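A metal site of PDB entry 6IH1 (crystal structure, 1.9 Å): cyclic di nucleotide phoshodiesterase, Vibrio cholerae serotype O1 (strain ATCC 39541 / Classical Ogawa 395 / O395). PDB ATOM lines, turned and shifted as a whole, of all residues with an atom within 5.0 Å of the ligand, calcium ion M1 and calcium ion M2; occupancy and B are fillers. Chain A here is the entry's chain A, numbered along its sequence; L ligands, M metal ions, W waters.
Calcium ion M2 is bound by the side-chain carboxylate of Asp 159, an oxygen (O2) of the ligand, the side-chain carboxylate of Glu 215 and the side-chain carboxylate of Asp 158.
Calcium ion M2 has four donor atoms within binding distance.
Slightly farther from calcium ion M2 lies water W4 (2.9 Å).
Slightly farther from calcium ion M2 lies the side-chain carboxylate (OE1) of Glu 215 (3.0 Å).
Slightly farther from calcium ion M2 lies OD2 of Asp 158 (3.1 Å).
Three residues have an atom within 4 Å of calcium ion M2: Asp 158, Asp 159 and Glu 215.
Calcium ion M1 is bound by the side-chain carboxylate of Glu 128, water W4, the side-chain amide oxygen of Asn 95, the side-chain carboxylate of Glu 45, the side-chain carboxylate of Asp 158 and an oxygen (O1) of the ligand.
Calcium ion M1 has six donor atoms within binding distance.
The backbone NH of Val 48 sits at hydrogen-bond distance from a nitrogen (N7) of the ligand (3.2 Å).
OH of Tyr 237 is in hydrogen-bond range of N5 of the ligand.
The side-chain sulfur of Met 182 sits close to a nitrogen (N4) of the ligand (3.8 Å).
O7 of the ligand lies within hydrogen-bond range of N of Tyr 237 (2.8 Å).
NH1 of Arg 49 is in salt-bridge range of O9 of the ligand, at 2.7 Å.
OE1 of Glu 218 is in hydrogen-bond range of N3 of the ligand (2.7 Å).
A nitrogen (N2) of the ligand lies within hydrogen-bond range of the side-chain amide nitrogen of Gln 31, at 3.0 Å.
SG of Cys 75 is in hydrogen-bond range of O14 of the ligand (3.7 Å).
The nearest printed residue that does not touch calcium ion M1 is Lys 179 (4.1 Å).
Water W4 lies within hydrogen-bond range of OE1 of Glu 45, NZ of Lys 179 and O3 of the ligand.
Water W3 lies within hydrogen-bond range of O14 of the ligand (2.7 Å), N of Asn 95 (2.8 Å) and O of Ala 46 (2.9 Å).
Water W7 bridges O8 of the ligand (2.7 Å) and N of Ala 56 (3.4 Å).
Water W6 lies within hydrogen-bond range of N2 of the ligand (2.8 Å), N of Gly 216 (3.0 Å) and O of Gln 235 (3.4 Å).
Water W2 bridges N10 of the ligand (3.0 Å) and O of Phe 96 (3.3 Å).
Water W1 lies within hydrogen-bond range of a nitrogen (N4) of the ligand and the side-chain carboxylate of Glu 218.
A nitrogen (N9) of the ligand sits close to the backbone NH of Leu 97, at 3.4 Å.
Merely in contact with the ligand: Pro 242 (3.3 Å), Gly 216 (3.4 Å), Gly 236 (3.4 Å), Val 217 (3.5 Å), Met 28 (3.5 Å), Ala 56 (3.5 Å), Ile 60 (3.6 Å), Leu 47 (3.7 Å), Phe 96 (3.8 Å) and Asp 72 (3.8 Å).
22 residues have an atom within 4 Å of the ligand: Met 28, Gln 31, Glu 45, Leu 47, Val 48, Arg 49, Ala 56, Ile 60, Asp 72, Cys 75, Asn 95, Phe 96, Leu 97, Asp 158, Asp 159, Met 182, Gly 216, Val 217, Glu 218, Gly 236, Tyr 237 and Pro 242.
N of Phe 96 is in hydrogen-bond range of O of Glu 128, at 2.9 Å.
The side-chain amino group (NZ) of Lys 179 lies within salt-bridge range of the side-chain carboxylate (OE1) of Glu 45 (3.2 Å).
The guanidinium group (NH2) of Arg 186 lies within hydrogen-bond range of the backbone carbonyl oxygen (O) of Gly 216 (2.8 Å).
The backbone NH (N) of Val 217 sits at hydrogen-bond distance from the backbone carbonyl oxygen (O) of Gln 235, 3.0 Å away.
The backbone NH (N) of Tyr 238 sits at hydrogen-bond distance from the backbone carbonyl oxygen (O) of Val 217 (3.0 Å).
The backbone NH (N) of Asp 159 lies within hydrogen-bond range of the backbone carbonyl oxygen (O) of Lys 179 (3.3 Å).
OE1 of Glu 45 sits at hydrogen-bond distance from NE2 of Gln 235.
The side-chain amide nitrogen (ND2) of Asn 95 lies within hydrogen-bond range of the backbone carbonyl oxygen (O) of Ala 46 (3.3 Å).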
ATOM      1  N   MET A  28     -24.982  27.361  27.216  1.00  0.00           N
ATOM      2  CA  MET A  28     -24.919  26.067  26.562  1.00  0.00           C
ATOM      3  C   MET A  28     -25.714  26.080  25.264  1.00  0.00           C
ATOM      4  O   MET A  28     -26.746  26.749  25.160  1.00  0.00           O
ATOM      5  CB  MET A  28     -25.472  24.958  27.486  1.00  0.00           C
ATOM      6  CG  MET A  28     -24.581  24.648  28.680  1.00  0.00           C
ATOM      7  SD  MET A  28     -23.089  23.781  28.141  1.00  0.00           S
ATOM      8  CE  MET A  28     -22.031  24.059  29.559  1.00  0.00           C
ATOM      9  N   GLN A  31     -27.207  19.617  21.200  1.00  0.00           N
ATOM     10  CA  GLN A  31     -27.272  18.951  19.925  1.00  0.00           C
ATOM     11  C   GLN A  31     -27.910  17.588  20.088  1.00  0.00           C
ATOM     12  O   GLN A  31     -27.438  16.790  20.926  1.00  0.00           O
ATOM     13  CB  GLN A  31     -25.873  18.785  19.274  1.00  0.00           C
ATOM     14  CG  GLN A  31     -25.941  18.300  17.801  1.00  0.00           C
ATOM     15  CD  GLN A  31     -24.571  18.057  17.164  1.00  0.00           C
ATOM     16  OE1 GLN A  31     -23.618  17.692  17.838  1.00  0.00           O
ATOM     17  NE2 GLN A  31     -24.478  18.295  15.851  1.00  0.00           N
ATOM     18  N   GLU A  45     -26.568  16.414  23.613  1.00  0.00           N
ATOM     19  CA  GLU A  45     -25.280  16.779  24.185  1.00  0.00           C
ATOM     20  C   GLU A  45     -25.267  18.269  24.491  1.00  0.00           C
ATOM     21  O   GLU A  45     -25.581  19.106  23.621  1.00  0.00           O
ATOM     22  CB  GLU A  45     -24.113  16.417  23.252  1.00  0.00           C
ATOM     23  CG  GLU A  45     -22.763  16.708  23.917  1.00  0.00           C
ATOM     24  CD  GLU A  45     -21.533  16.393  23.060  1.00  0.00           C
ATOM     25  OE1 GLU A  45     -21.654  15.987  21.867  1.00  0.00           O
ATOM     26  OE2 GLU A  45     -20.415  16.588  23.608  1.00  0.00           O
ATOM     27  N   ALA A  46     -24.884  18.612  25.726  1.00  0.00           N
ATOM     28  CA  ALA A  46     -24.667  20.010  26.077  1.00  0.00           C
ATOM     29  C   ALA A  46     -23.287  20.440  25.623  1.00  0.00           C
ATOM     30  O   ALA A  46     -22.291  19.749  25.883  1.00  0.00           O
ATOM     31  CB  ALA A  46     -24.827  20.231  27.576  1.00  0.00           C
ATOM     32  N   LEU A  47     -23.225  21.587  24.951  1.00  0.00           N
ATOM     33  CA  LEU A  47     -21.988  22.103  24.392  1.00  0.00           C
ATOM     34  C   LEU A  47     -21.835  23.553  24.831  1.00  0.00           C
ATOM     35  O   LEU A  47     -22.707  24.380  24.556  1.00  0.00           O
ATOM     36  CB  LEU A  47     -21.980  21.997  22.855  1.00  0.00           C
ATOM     37  CG  LEU A  47     -22.040  20.554  22.352  1.00  0.00           C
ATOM     38  CD1 LEU A  47     -22.439  20.495  20.875  1.00  0.00           C
ATOM     39  CD2 LEU A  47     -20.690  19.892  22.577  1.00  0.00           C
ATOM     40  N   VAL A  48     -20.723  23.856  25.502  1.00  0.00           N
ATOM     41  CA  VAL A  48     -20.530  25.162  26.109  1.00  0.00           C
ATOM     42  C   VAL A  48     -20.386  26.221  25.024  1.00  0.00           C
ATOM     43  O   VAL A  48     -19.726  26.001  23.987  1.00  0.00           O
ATOM     44  CB  VAL A  48     -19.324  25.134  27.064  1.00  0.00           C
ATOM     45  CG1 VAL A  48     -18.028  24.890  26.308  1.00  0.00           C
ATOM     46  CG2 VAL A  48     -19.229  26.440  27.826  1.00  0.00           C
ATOM     47  N   ARG A  49     -21.004  27.388  25.260  1.00  0.00           N
ATOM     48  CA  ARG A  49     -20.969  28.522  24.351  1.00  0.00           C
ATOM     49  C   ARG A  49     -20.766  29.800  25.143  1.00  0.00           C
ATOM     50  O   ARG A  49     -21.036  29.856  26.347  1.00  0.00           O
ATOM     51  CB  ARG A  49     -22.263  28.630  23.543  1.00  0.00           C
ATOM     52  CG  ARG A  49     -22.519  27.464  22.617  1.00  0.00           C
ATOM     53  CD  ARG A  49     -21.596  27.545  21.418  1.00  0.00           C
ATOM     54  NE  ARG A  49     -21.853  26.492  20.447  1.00  0.00           N
ATOM     55  CZ  ARG A  49     -21.240  25.309  20.432  1.00  0.00           C
ATOM     56  NH1 ARG A  49     -20.326  25.025  21.368  1.00  0.00           N
ATOM     57  NH2 ARG A  49     -21.536  24.416  19.493  1.00  0.00           N
ATOM     58  N   ALA A  56     -17.013  27.136  21.715  1.00  0.00           N
ATOM     59  CA  ALA A  56     -16.613  26.423  22.937  1.00  0.00           C
ATOM     60  C   ALA A  56     -15.134  26.617  23.251  1.00  0.00           C
ATOM     61  O   ALA A  56     -14.765  26.775  24.422  1.00  0.00           O
ATOM     62  CB  ALA A  56     -16.927  24.926  22.780  1.00  0.00           C
ATOM     63  N   ILE A  60     -13.486  27.783  26.691  1.00  0.00           N
ATOM     64  CA  ILE A  60     -12.564  26.908  27.400  1.00  0.00           C
ATOM     65  C   ILE A  60     -11.158  27.507  27.428  1.00  0.00           C
ATOM     66  O   ILE A  60     -10.385  27.224  28.342  1.00  0.00           O
ATOM     67  CB  ILE A  60     -12.595  25.510  26.744  1.00  0.00           C
ATOM     68  CG1 ILE A  60     -13.996  24.907  26.905  1.00  0.00           C
ATOM     69  CG2 ILE A  60     -11.545  24.586  27.334  1.00  0.00           C
ATOM     70  CD1 ILE A  60     -14.172  23.544  26.259  1.00  0.00           C
ATOM     71  N   PHE A  71     -15.200  25.904  36.805  1.00  0.00           N
ATOM     72  CA  PHE A  71     -15.751  25.880  35.448  1.00  0.00           C
ATOM     73  C   PHE A  71     -16.530  24.606  35.182  1.00  0.00           C
ATOM     74  O   PHE A  71     -17.606  24.629  34.575  1.00  0.00           O
ATOM     75  CB  PHE A  71     -14.640  26.061  34.420  1.00  0.00           C
ATOM     76  CG  PHE A  71     -15.080  25.811  32.994  1.00  0.00           C
ATOM     77  CD1 PHE A  71     -15.772  26.785  32.296  1.00  0.00           C
ATOM     78  CD2 PHE A  71     -14.793  24.612  32.364  1.00  0.00           C
ATOM     79  CE1 PHE A  71     -16.174  26.569  30.996  1.00  0.00           C
ATOM     80  CE2 PHE A  71     -15.189  24.387  31.056  1.00  0.00           C
ATOM     81  CZ  PHE A  71     -15.884  25.366  30.374  1.00  0.00           C
ATOM     82  N   ASP A  72     -15.975  23.458  35.602  1.00  0.00           N
ATOM     83  CA  ASP A  72     -16.657  22.189  35.378  1.00  0.00           C
ATOM     84  C   ASP A  72     -17.991  22.126  36.106  1.00  0.00           C
ATOM     85  O   ASP A  72     -18.976  21.615  35.574  1.00  0.00           O
ATOM     86  CB  ASP A  72     -15.759  21.034  35.830  1.00  0.00           C
ATOM     87  CG  ASP A  72     -16.117  19.728  35.173  1.00  0.00           C
ATOM     88  OD1 ASP A  72     -15.922  19.605  33.945  1.00  0.00           O
ATOM     89  OD2 ASP A  72     -16.616  18.826  35.870  1.00  0.00           O
ATOM     90  N   CYS A  75     -20.603  24.267  34.227  1.00  0.00           N
ATOM     91  CA  CYS A  75     -21.087  23.601  33.026  1.00  0.00           C
ATOM     92  C   CYS A  75     -22.233  22.658  33.338  1.00  0.00           C
ATOM     93  O   CYS A  75     -23.261  22.655  32.650  1.00  0.00           O
ATOM     94  CB  CYS A  75     -19.946  22.847  32.324  1.00  0.00           C
ATOM     95  SG  CYS A  75     -18.721  23.856  31.435  1.00  0.00           S
ATOM     96  N   ASN A  95     -20.126  16.887  28.891  1.00  0.00           N
ATOM     97  CA  ASN A  95     -18.710  16.589  28.734  1.00  0.00           C
ATOM     98  C   ASN A  95     -17.995  16.738  30.068  1.00  0.00           C
ATOM     99  O   ASN A  95     -18.227  17.697  30.808  1.00  0.00           O
ATOM    100  CB  ASN A  95     -18.069  17.497  27.703  1.00  0.00           C
ATOM    101  CG  ASN A  95     -18.549  17.204  26.302  1.00  0.00           C
ATOM    102  OD1 ASN A  95     -18.153  16.194  25.704  1.00  0.00           O
ATOM    103  ND2 ASN A  95     -19.425  18.073  25.777  1.00  0.00           N
ATOM    104  N   PHE A  96     -17.133  15.778  30.367  1.00  0.00           N
ATOM    105  CA  PHE A  96     -16.324  15.769  31.567  1.00  0.00           C
ATOM    106  C   PHE A  96     -14.949  16.317  31.241  1.00  0.00           C
ATOM    107  O   PHE A  96     -14.330  15.905  30.254  1.00  0.00           O
ATOM    108  CB  PHE A  96     -16.237  14.345  32.127  1.00  0.00           C
ATOM    109  CG  PHE A  96     -15.518  14.239  33.435  1.00  0.00           C
ATOM    110  CD1 PHE A  96     -14.135  14.069  33.458  1.00  0.00           C
ATOM    111  CD2 PHE A  96     -16.208  14.265  34.625  1.00  0.00           C
ATOM    112  CE1 PHE A  96     -13.454  13.956  34.656  1.00  0.00           C
ATOM    113  CE2 PHE A  96     -15.533  14.149  35.836  1.00  0.00           C
ATOM    114  CZ  PHE A  96     -14.162  13.998  35.849  1.00  0.00           C
ATOM    115  N   LEU A  97     -14.488  17.265  32.057  1.00  0.00           N
ATOM    116  CA  LEU A  97     -13.235  17.962  31.774  1.00  0.00           C
ATOM    117  C   LEU A  97     -12.079  16.962  31.828  1.00  0.00           C
ATOM    118  O   LEU A  97     -12.015  16.143  32.748  1.00  0.00           O
ATOM    119  CB  LEU A  97     -13.041  19.094  32.774  1.00  0.00           C
ATOM    120  CG  LEU A  97     -12.099  20.280  32.514  1.00  0.00           C
ATOM    121  CD1 LEU A  97     -12.497  21.032  31.253  1.00  0.00           C
ATOM    122  CD2 LEU A  97     -12.116  21.217  33.706  1.00  0.00           C
ATOM    123  N   PRO A  98     -11.126  17.023  30.883  1.00  0.00           N
ATOM    124  CA  PRO A  98     -10.140  15.933  30.754  1.00  0.00           C
ATOM    125  C   PRO A  98      -9.346  15.607  32.010  1.00  0.00           C
ATOM    126  O   PRO A  98      -9.319  14.445  32.438  1.00  0.00           O
ATOM    127  CB  PRO A  98      -9.221  16.432  29.624  1.00  0.00           C
ATOM    128  CG  PRO A  98      -9.481  17.904  29.511  1.00  0.00           C
ATOM    129  CD  PRO A  98     -10.910  18.102  29.904  1.00  0.00           C
ATOM    130  N   GLU A 128     -19.540  12.221  29.383  1.00  0.00           N
ATOM    131  CA  GLU A 128     -18.666  11.824  28.293  1.00  0.00           C
ATOM    132  C   GLU A 128     -17.222  12.022  28.729  1.00  0.00           C
ATOM    133  O   GLU A 128     -16.866  13.110  29.181  1.00  0.00           O
ATOM    134  CB  GLU A 128     -18.974  12.617  27.024  1.00  0.00           C
ATOM    135  CG  GLU A 128     -20.425  12.469  26.606  1.00  0.00           C
ATOM    136  CD  GLU A 128     -20.748  13.109  25.256  1.00  0.00           C
ATOM    137  OE1 GLU A 128     -21.942  13.070  24.858  1.00  0.00           O
ATOM    138  OE2 GLU A 128     -19.815  13.606  24.588  1.00  0.00           O
ATOM    139  N   ASP A 158     -15.735   9.332  24.888  1.00  0.00           N
ATOM    140  CA  ASP A 158     -15.884  10.275  23.804  1.00  0.00           C
ATOM    141  C   ASP A 158     -14.681  10.196  22.850  1.00  0.00           C
ATOM    142  O   ASP A 158     -13.575   9.819  23.247  1.00  0.00           O
ATOM    143  CB  ASP A 158     -16.028  11.673  24.389  1.00  0.00           C
ATOM    144  CG  ASP A 158     -16.615  12.660  23.421  1.00  0.00           C
ATOM    145  OD1 ASP A 158     -17.123  12.241  22.355  1.00  0.00           O
ATOM    146  OD2 ASP A 158     -16.600  13.861  23.732  1.00  0.00           O
ATOM    147  N   ASP A 159     -14.908  10.567  21.590  1.00  0.00           N
ATOM    148  CA  ASP A 159     -13.824  10.672  20.601  1.00  0.00           C
ATOM    149  C   ASP A 159     -13.018   9.386  20.460  1.00  0.00           C
ATOM    150  O   ASP A 159     -11.798   9.401  20.320  1.00  0.00           O
ATOM    151  CB  ASP A 159     -12.897  11.837  20.945  1.00  0.00           C
ATOM    152  CG  ASP A 159     -13.601  13.170  20.873  1.00  0.00           C
ATOM    153  OD1 ASP A 159     -14.595  13.272  20.125  1.00  0.00           O
ATOM    154  OD2 ASP A 159     -13.158  14.116  21.551  1.00  0.00           O
ATOM    155  N   LYS A 179     -18.746   6.788  21.903  1.00  0.00           N
ATOM    156  CA  LYS A 179     -18.955   7.708  20.791  1.00  0.00           C
ATOM    157  C   LYS A 179     -17.732   7.609  19.890  1.00  0.00           C
ATOM    158  O   LYS A 179     -16.635   8.029  20.284  1.00  0.00           O
ATOM    159  CB  LYS A 179     -19.167   9.136  21.284  1.00  0.00           C
ATOM    160  CG  LYS A 179     -20.229   9.245  22.422  1.00  0.00           C
ATOM    161  CD  LYS A 179     -20.482  10.699  22.837  1.00  0.00           C
ATOM    162  CE  LYS A 179     -21.357  11.382  21.799  1.00  0.00           C
ATOM    163  NZ  LYS A 179     -21.624  12.789  22.096  1.00  0.00           N
ATOM    164  N   MET A 182     -15.527  11.396  14.766  1.00  0.00           N
ATOM    165  CA  MET A 182     -16.007  11.692  13.433  1.00  0.00           C
ATOM    166  C   MET A 182     -14.949  11.414  12.369  1.00  0.00           C
ATOM    167  O   MET A 182     -15.308  11.115  11.223  1.00  0.00           O
ATOM    168  CB  MET A 182     -16.490  13.137  13.348  1.00  0.00           C
ATOM    169  CG  MET A 182     -15.430  14.190  13.583  1.00  0.00           C
ATOM    170  SD  MET A 182     -16.187  15.817  13.562  1.00  0.00           S
ATOM    171  CE  MET A 182     -17.332  15.669  14.932  1.00  0.00           C
ATOM    172  N   ARG A 186     -16.068   9.790   8.716  1.00  0.00           N
ATOM    173  CA  ARG A 186     -16.123  10.659   7.545  1.00  0.00           C
ATOM    174  C   ARG A 186     -16.017   9.846   6.260  1.00  0.00           C
ATOM    175  O   ARG A 186     -15.049   9.100   6.068  1.00  0.00           O
ATOM    176  CB  ARG A 186     -15.013  11.707   7.593  1.00  0.00           C
ATOM    177  CG  ARG A 186     -15.070  12.758   6.453  1.00  0.00           C
ATOM    178  CD  ARG A 186     -16.331  13.593   6.547  1.00  0.00           C
ATOM    179  NE  ARG A 186     -16.506  14.190   7.879  1.00  0.00           N
ATOM    180  CZ  ARG A 186     -17.540  13.960   8.697  1.00  0.00           C
ATOM    181  NH1 ARG A 186     -18.541  13.150   8.361  1.00  0.00           N
ATOM    182  NH2 ARG A 186     -17.578  14.561   9.887  1.00  0.00           N
ATOM    183  N   GLU A 215     -20.595   9.791  15.699  1.00  0.00           N
ATOM    184  CA  GLU A 215     -20.541  11.226  15.864  1.00  0.00           C
ATOM    185  C   GLU A 215     -20.081  11.867  14.566  1.00  0.00           C
ATOM    186  O   GLU A 215     -19.387  11.251  13.750  1.00  0.00           O
ATOM    187  CB  GLU A 215     -19.582  11.529  17.020  1.00  0.00           C
ATOM    188  CG  GLU A 215     -19.511  12.938  17.488  1.00  0.00           C
ATOM    189  CD  GLU A 215     -18.872  12.995  18.856  1.00  0.00           C
ATOM    190  OE1 GLU A 215     -19.544  13.481  19.795  1.00  0.00           O
ATOM    191  OE2 GLU A 215     -17.725  12.505  19.009  1.00  0.00           O
ATOM    192  N   GLY A 216     -20.492  13.109  14.365  1.00  0.00           N
ATOM    193  CA  GLY A 216     -20.072  13.901  13.225  1.00  0.00           C
ATOM    194  C   GLY A 216     -20.647  13.452  11.890  1.00  0.00           C
ATOM    195  O   GLY A 216     -20.044  13.723  10.849  1.00  0.00           O
ATOM    196  N   VAL A 217     -21.819  12.806  11.886  1.00  0.00           N
ATOM    197  CA  VAL A 217     -22.431  12.378  10.636  1.00  0.00           C
ATOM    198  C   VAL A 217     -22.867  13.612   9.875  1.00  0.00           C
ATOM    199  O   VAL A 217     -23.593  14.455  10.410  1.00  0.00           O
ATOM    200  CB  VAL A 217     -23.625  11.445  10.886  1.00  0.00           C
ATOM    201  CG1 VAL A 217     -24.308  11.052   9.560  1.00  0.00           C
ATOM    202  CG2 VAL A 217     -23.167  10.232  11.663  1.00  0.00           C
ATOM    203  N   GLU A 218     -22.402  13.752   8.617  1.00  0.00           N
ATOM    204  CA  GLU A 218     -22.657  14.945   7.830  1.00  0.00           C
ATOM    205  C   GLU A 218     -23.491  14.721   6.579  1.00  0.00           C
ATOM    206  O   GLU A 218     -23.946  15.700   5.993  1.00  0.00           O
ATOM    207  CB  GLU A 218     -21.325  15.633   7.454  1.00  0.00           C
ATOM    208  CG  GLU A 218     -20.668  16.315   8.640  1.00  0.00           C
ATOM    209  CD  GLU A 218     -19.358  16.998   8.292  1.00  0.00           C
ATOM    210  OE1 GLU A 218     -18.717  17.593   9.195  1.00  0.00           O
ATOM    211  OE2 GLU A 218     -18.949  16.918   7.110  1.00  0.00           O
ATOM    212  N   GLN A 235     -25.181  11.238  15.759  1.00  0.00           N
ATOM    213  CA  GLN A 235     -25.120  12.648  16.075  1.00  0.00           C
ATOM    214  C   GLN A 235     -24.386  13.332  14.934  1.00  0.00           C
ATOM    215  O   GLN A 235     -23.429  12.777  14.396  1.00  0.00           O
ATOM    216  CB  GLN A 235     -24.395  12.850  17.412  1.00  0.00           C
ATOM    217  CG  GLN A 235     -24.439  14.261  17.993  1.00  0.00           C
ATOM    218  CD  GLN A 235     -23.697  14.379  19.324  1.00  0.00           C
ATOM    219  OE1 GLN A 235     -23.400  13.375  19.986  1.00  0.00           O
ATOM    220  NE2 GLN A 235     -23.442  15.621  19.741  1.00  0.00           N
ATOM    221  N   GLY A 236     -24.836  14.525  14.562  1.00  0.00           N
ATOM    222  CA  GLY A 236     -24.085  15.251  13.546  1.00  0.00           C
ATOM    223  C   GLY A 236     -24.936  16.269  12.821  1.00  0.00           C
ATOM    224  O   GLY A 236     -26.173  16.296  12.931  1.00  0.00           O
ATOM    225  N   TYR A 237     -24.239  17.100  12.050  1.00  0.00           N
ATOM    226  CA  TYR A 237     -24.875  18.144  11.252  1.00  0.00           C
ATOM    227  C   TYR A 237     -25.952  17.589  10.320  1.00  0.00           C
ATOM    228  O   TYR A 237     -26.915  18.292  10.007  1.00  0.00           O
ATOM    229  CB  TYR A 237     -23.828  18.915  10.446  1.00  0.00           C
ATOM    230  CG  TYR A 237     -22.856  19.713  11.301  1.00  0.00           C
ATOM    231  CD1 TYR A 237     -23.156  20.012  12.628  1.00  0.00           C
ATOM    232  CD2 TYR A 237     -21.645  20.188  10.774  1.00  0.00           C
ATOM    233  CE1 TYR A 237     -22.278  20.746  13.419  1.00  0.00           C
ATOM    234  CE2 TYR A 237     -20.757  20.934  11.556  1.00  0.00           C
ATOM    235  CZ  TYR A 237     -21.094  21.211  12.884  1.00  0.00           C
ATOM    236  OH  TYR A 237     -20.231  21.942  13.691  1.00  0.00           O
ATOM    237  N   TYR A 238     -25.812  16.335   9.878  1.00  0.00           N
ATOM    238  CA  TYR A 238     -26.839  15.726   9.029  1.00  0.00           C
ATOM    239  C   TYR A 238     -28.203  15.725   9.719  1.00  0.00           C
ATOM    240  O   TYR A 238     -29.233  15.944   9.073  1.00  0.00           O
ATOM    241  CB  TYR A 238     -26.442  14.292   8.636  1.00  0.00           C
ATOM    242  CG  TYR A 238     -27.520  13.658   7.779  1.00  0.00           C
ATOM    243  CD1 TYR A 238     -27.815  14.183   6.535  1.00  0.00           C
ATOM    244  CD2 TYR A 238     -28.250  12.560   8.218  1.00  0.00           C
ATOM    245  CE1 TYR A 238     -28.807  13.638   5.746  1.00  0.00           C
ATOM    246  CE2 TYR A 238     -29.229  11.995   7.438  1.00  0.00           C
ATOM    247  CZ  TYR A 238     -29.497  12.530   6.202  1.00  0.00           C
ATOM    248  OH  TYR A 238     -30.495  11.982   5.425  1.00  0.00           O
ATOM    249  N   PRO A 242     -25.870  22.069  16.587  1.00  0.00           N
ATOM    250  CA  PRO A 242     -26.130  22.481  17.965  1.00  0.00           C
ATOM    251  C   PRO A 242     -26.999  23.732  17.976  1.00  0.00           C
ATOM    252  O   PRO A 242     -26.849  24.621  17.141  1.00  0.00           O
ATOM    253  CB  PRO A 242     -24.729  22.766  18.525  1.00  0.00           C
ATOM    254  CG  PRO A 242     -23.816  21.924  17.685  1.00  0.00           C
ATOM    255  CD  PRO A 242     -24.420  21.974  16.306  1.00  0.00           C
HETATM  256  P1  LIG L   1     -16.924  17.226  21.301  1.00  0.00           P
HETATM  257  O1  LIG L   1     -17.026  16.580  22.664  1.00  0.00           O
HETATM  258  O2  LIG L   1     -16.461  16.141  20.350  1.00  0.00           O
HETATM  259  O3  LIG L   1     -18.383  17.760  20.671  1.00  0.00           O
HETATM  260  C1  LIG L   1     -18.611  17.637  19.230  1.00  0.00           C
HETATM  261  C2  LIG L   1     -18.133  18.725  18.572  1.00  0.00           C
HETATM  262  O4  LIG L   1     -18.276  18.543  17.069  1.00  0.00           O
HETATM  263  C3  LIG L   1     -19.016  20.045  18.879  1.00  0.00           C
HETATM  264  O5  LIG L   1     -18.142  21.275  18.572  1.00  0.00           O
HETATM  265  C4  LIG L   1     -19.937  19.959  18.060  1.00  0.00           C
HETATM  266  O6  LIG L   1     -20.553  21.278  17.818  1.00  0.00           O
HETATM  267  C5  LIG L   1     -19.232  19.355  16.660  1.00  0.00           C
HETATM  268  N1  LIG L   1     -20.204  18.628  15.930  1.00  0.00           N
HETATM  269  C6  LIG L   1     -21.385  18.015  16.068  1.00  0.00           C
HETATM  270  N2  LIG L   1     -21.718  17.481  14.889  1.00  0.00           N
HETATM  271  C7  LIG L   1     -20.755  17.747  14.019  1.00  0.00           C
HETATM  272  C8  LIG L   1     -20.605  17.393  12.545  1.00  0.00           C
HETATM  273  O7  LIG L   1     -21.448  16.757  12.001  1.00  0.00           O
HETATM  274  N3  LIG L   1     -19.452  17.798  11.808  1.00  0.00           N
HETATM  275  C9  LIG L   1     -18.431  18.552  12.489  1.00  0.00           C
HETATM  276  N4  LIG L   1     -17.266  18.965  11.752  1.00  0.00           N
HETATM  277  N5  LIG L   1     -18.572  18.904  13.910  1.00  0.00           N
HETATM  278  C10 LIG L   1     -19.779  18.466  14.660  1.00  0.00           C
HETATM  279  P2  LIG L   1     -18.062  22.408  19.840  1.00  0.00           P
HETATM  280  O8  LIG L   1     -17.383  23.715  19.488  1.00  0.00           O
HETATM  281  O9  LIG L   1     -19.475  22.719  20.279  1.00  0.00           O
HETATM  282  O10 LIG L   1     -17.347  21.500  21.023  1.00  0.00           O
HETATM  283  C11 LIG L   1     -15.967  21.370  20.721  1.00  0.00           C
HETATM  284  C12 LIG L   1     -15.317  20.570  21.892  1.00  0.00           C
HETATM  285  O11 LIG L   1     -15.358  21.438  23.257  1.00  0.00           O
HETATM  286  C13 LIG L   1     -16.023  19.580  22.144  1.00  0.00           C
HETATM  287  O12 LIG L   1     -15.685  18.387  21.200  1.00  0.00           O
HETATM  288  C14 LIG L   1     -15.666  19.243  23.641  1.00  0.00           C
HETATM  289  O13 LIG L   1     -14.566  18.432  23.725  1.00  0.00           O
HETATM  290  C15 LIG L   1     -15.376  20.579  24.231  1.00  0.00           C
HETATM  291  N6  LIG L   1     -16.421  20.904  25.281  1.00  0.00           N
HETATM  292  C16 LIG L   1     -17.481  21.435  24.630  1.00  0.00           C
HETATM  293  N7  LIG L   1     -18.408  21.714  25.589  1.00  0.00           N
HETATM  294  C17 LIG L   1     -17.901  21.355  26.781  1.00  0.00           C
HETATM  295  C18 LIG L   1     -18.436  21.416  28.237  1.00  0.00           C
HETATM  296  O14 LIG L   1     -19.517  21.844  28.434  1.00  0.00           O
HETATM  297  N8  LIG L   1     -17.630  20.944  29.321  1.00  0.00           N
HETATM  298  C19 LIG L   1     -16.301  20.407  29.072  1.00  0.00           C
HETATM  299  N9  LIG L   1     -15.465  19.912  30.157  1.00  0.00           N
HETATM  300  N10 LIG L   1     -15.794  20.352  27.702  1.00  0.00           N
HETATM  301  C20 LIG L   1     -16.645  20.844  26.584  1.00  0.00           C
HETATM  302 CA    CA M   1     -18.593  15.114  23.715  1.00  0.00          CA
HETATM  303 CA    CA M   2     -16.724  13.895  20.605  1.00  0.00          CA
HETATM  304  O   HOH W   1     -17.870  20.928   9.182  1.00  0.00           O
HETATM  305  O   HOH W   2     -13.734  18.252  27.974  1.00  0.00           O
HETATM  306  O   HOH W   3     -20.823  19.488  28.331  1.00  0.00           O
HETATM  307  O   HOH W   4     -19.320  14.767  21.591  1.00  0.00           O
HETATM  308  O   HOH W   5     -16.053  19.982  14.599  1.00  0.00           O
HETATM  309  O   HOH W   6     -21.751  15.105  16.297  1.00  0.00           O
HETATM  310  O   HOH W   7     -18.311  26.150  18.735  1.00  0.00           O
HETATM  311  O   HOH W   8     -17.171  21.860  12.448  1.00  0.00           O
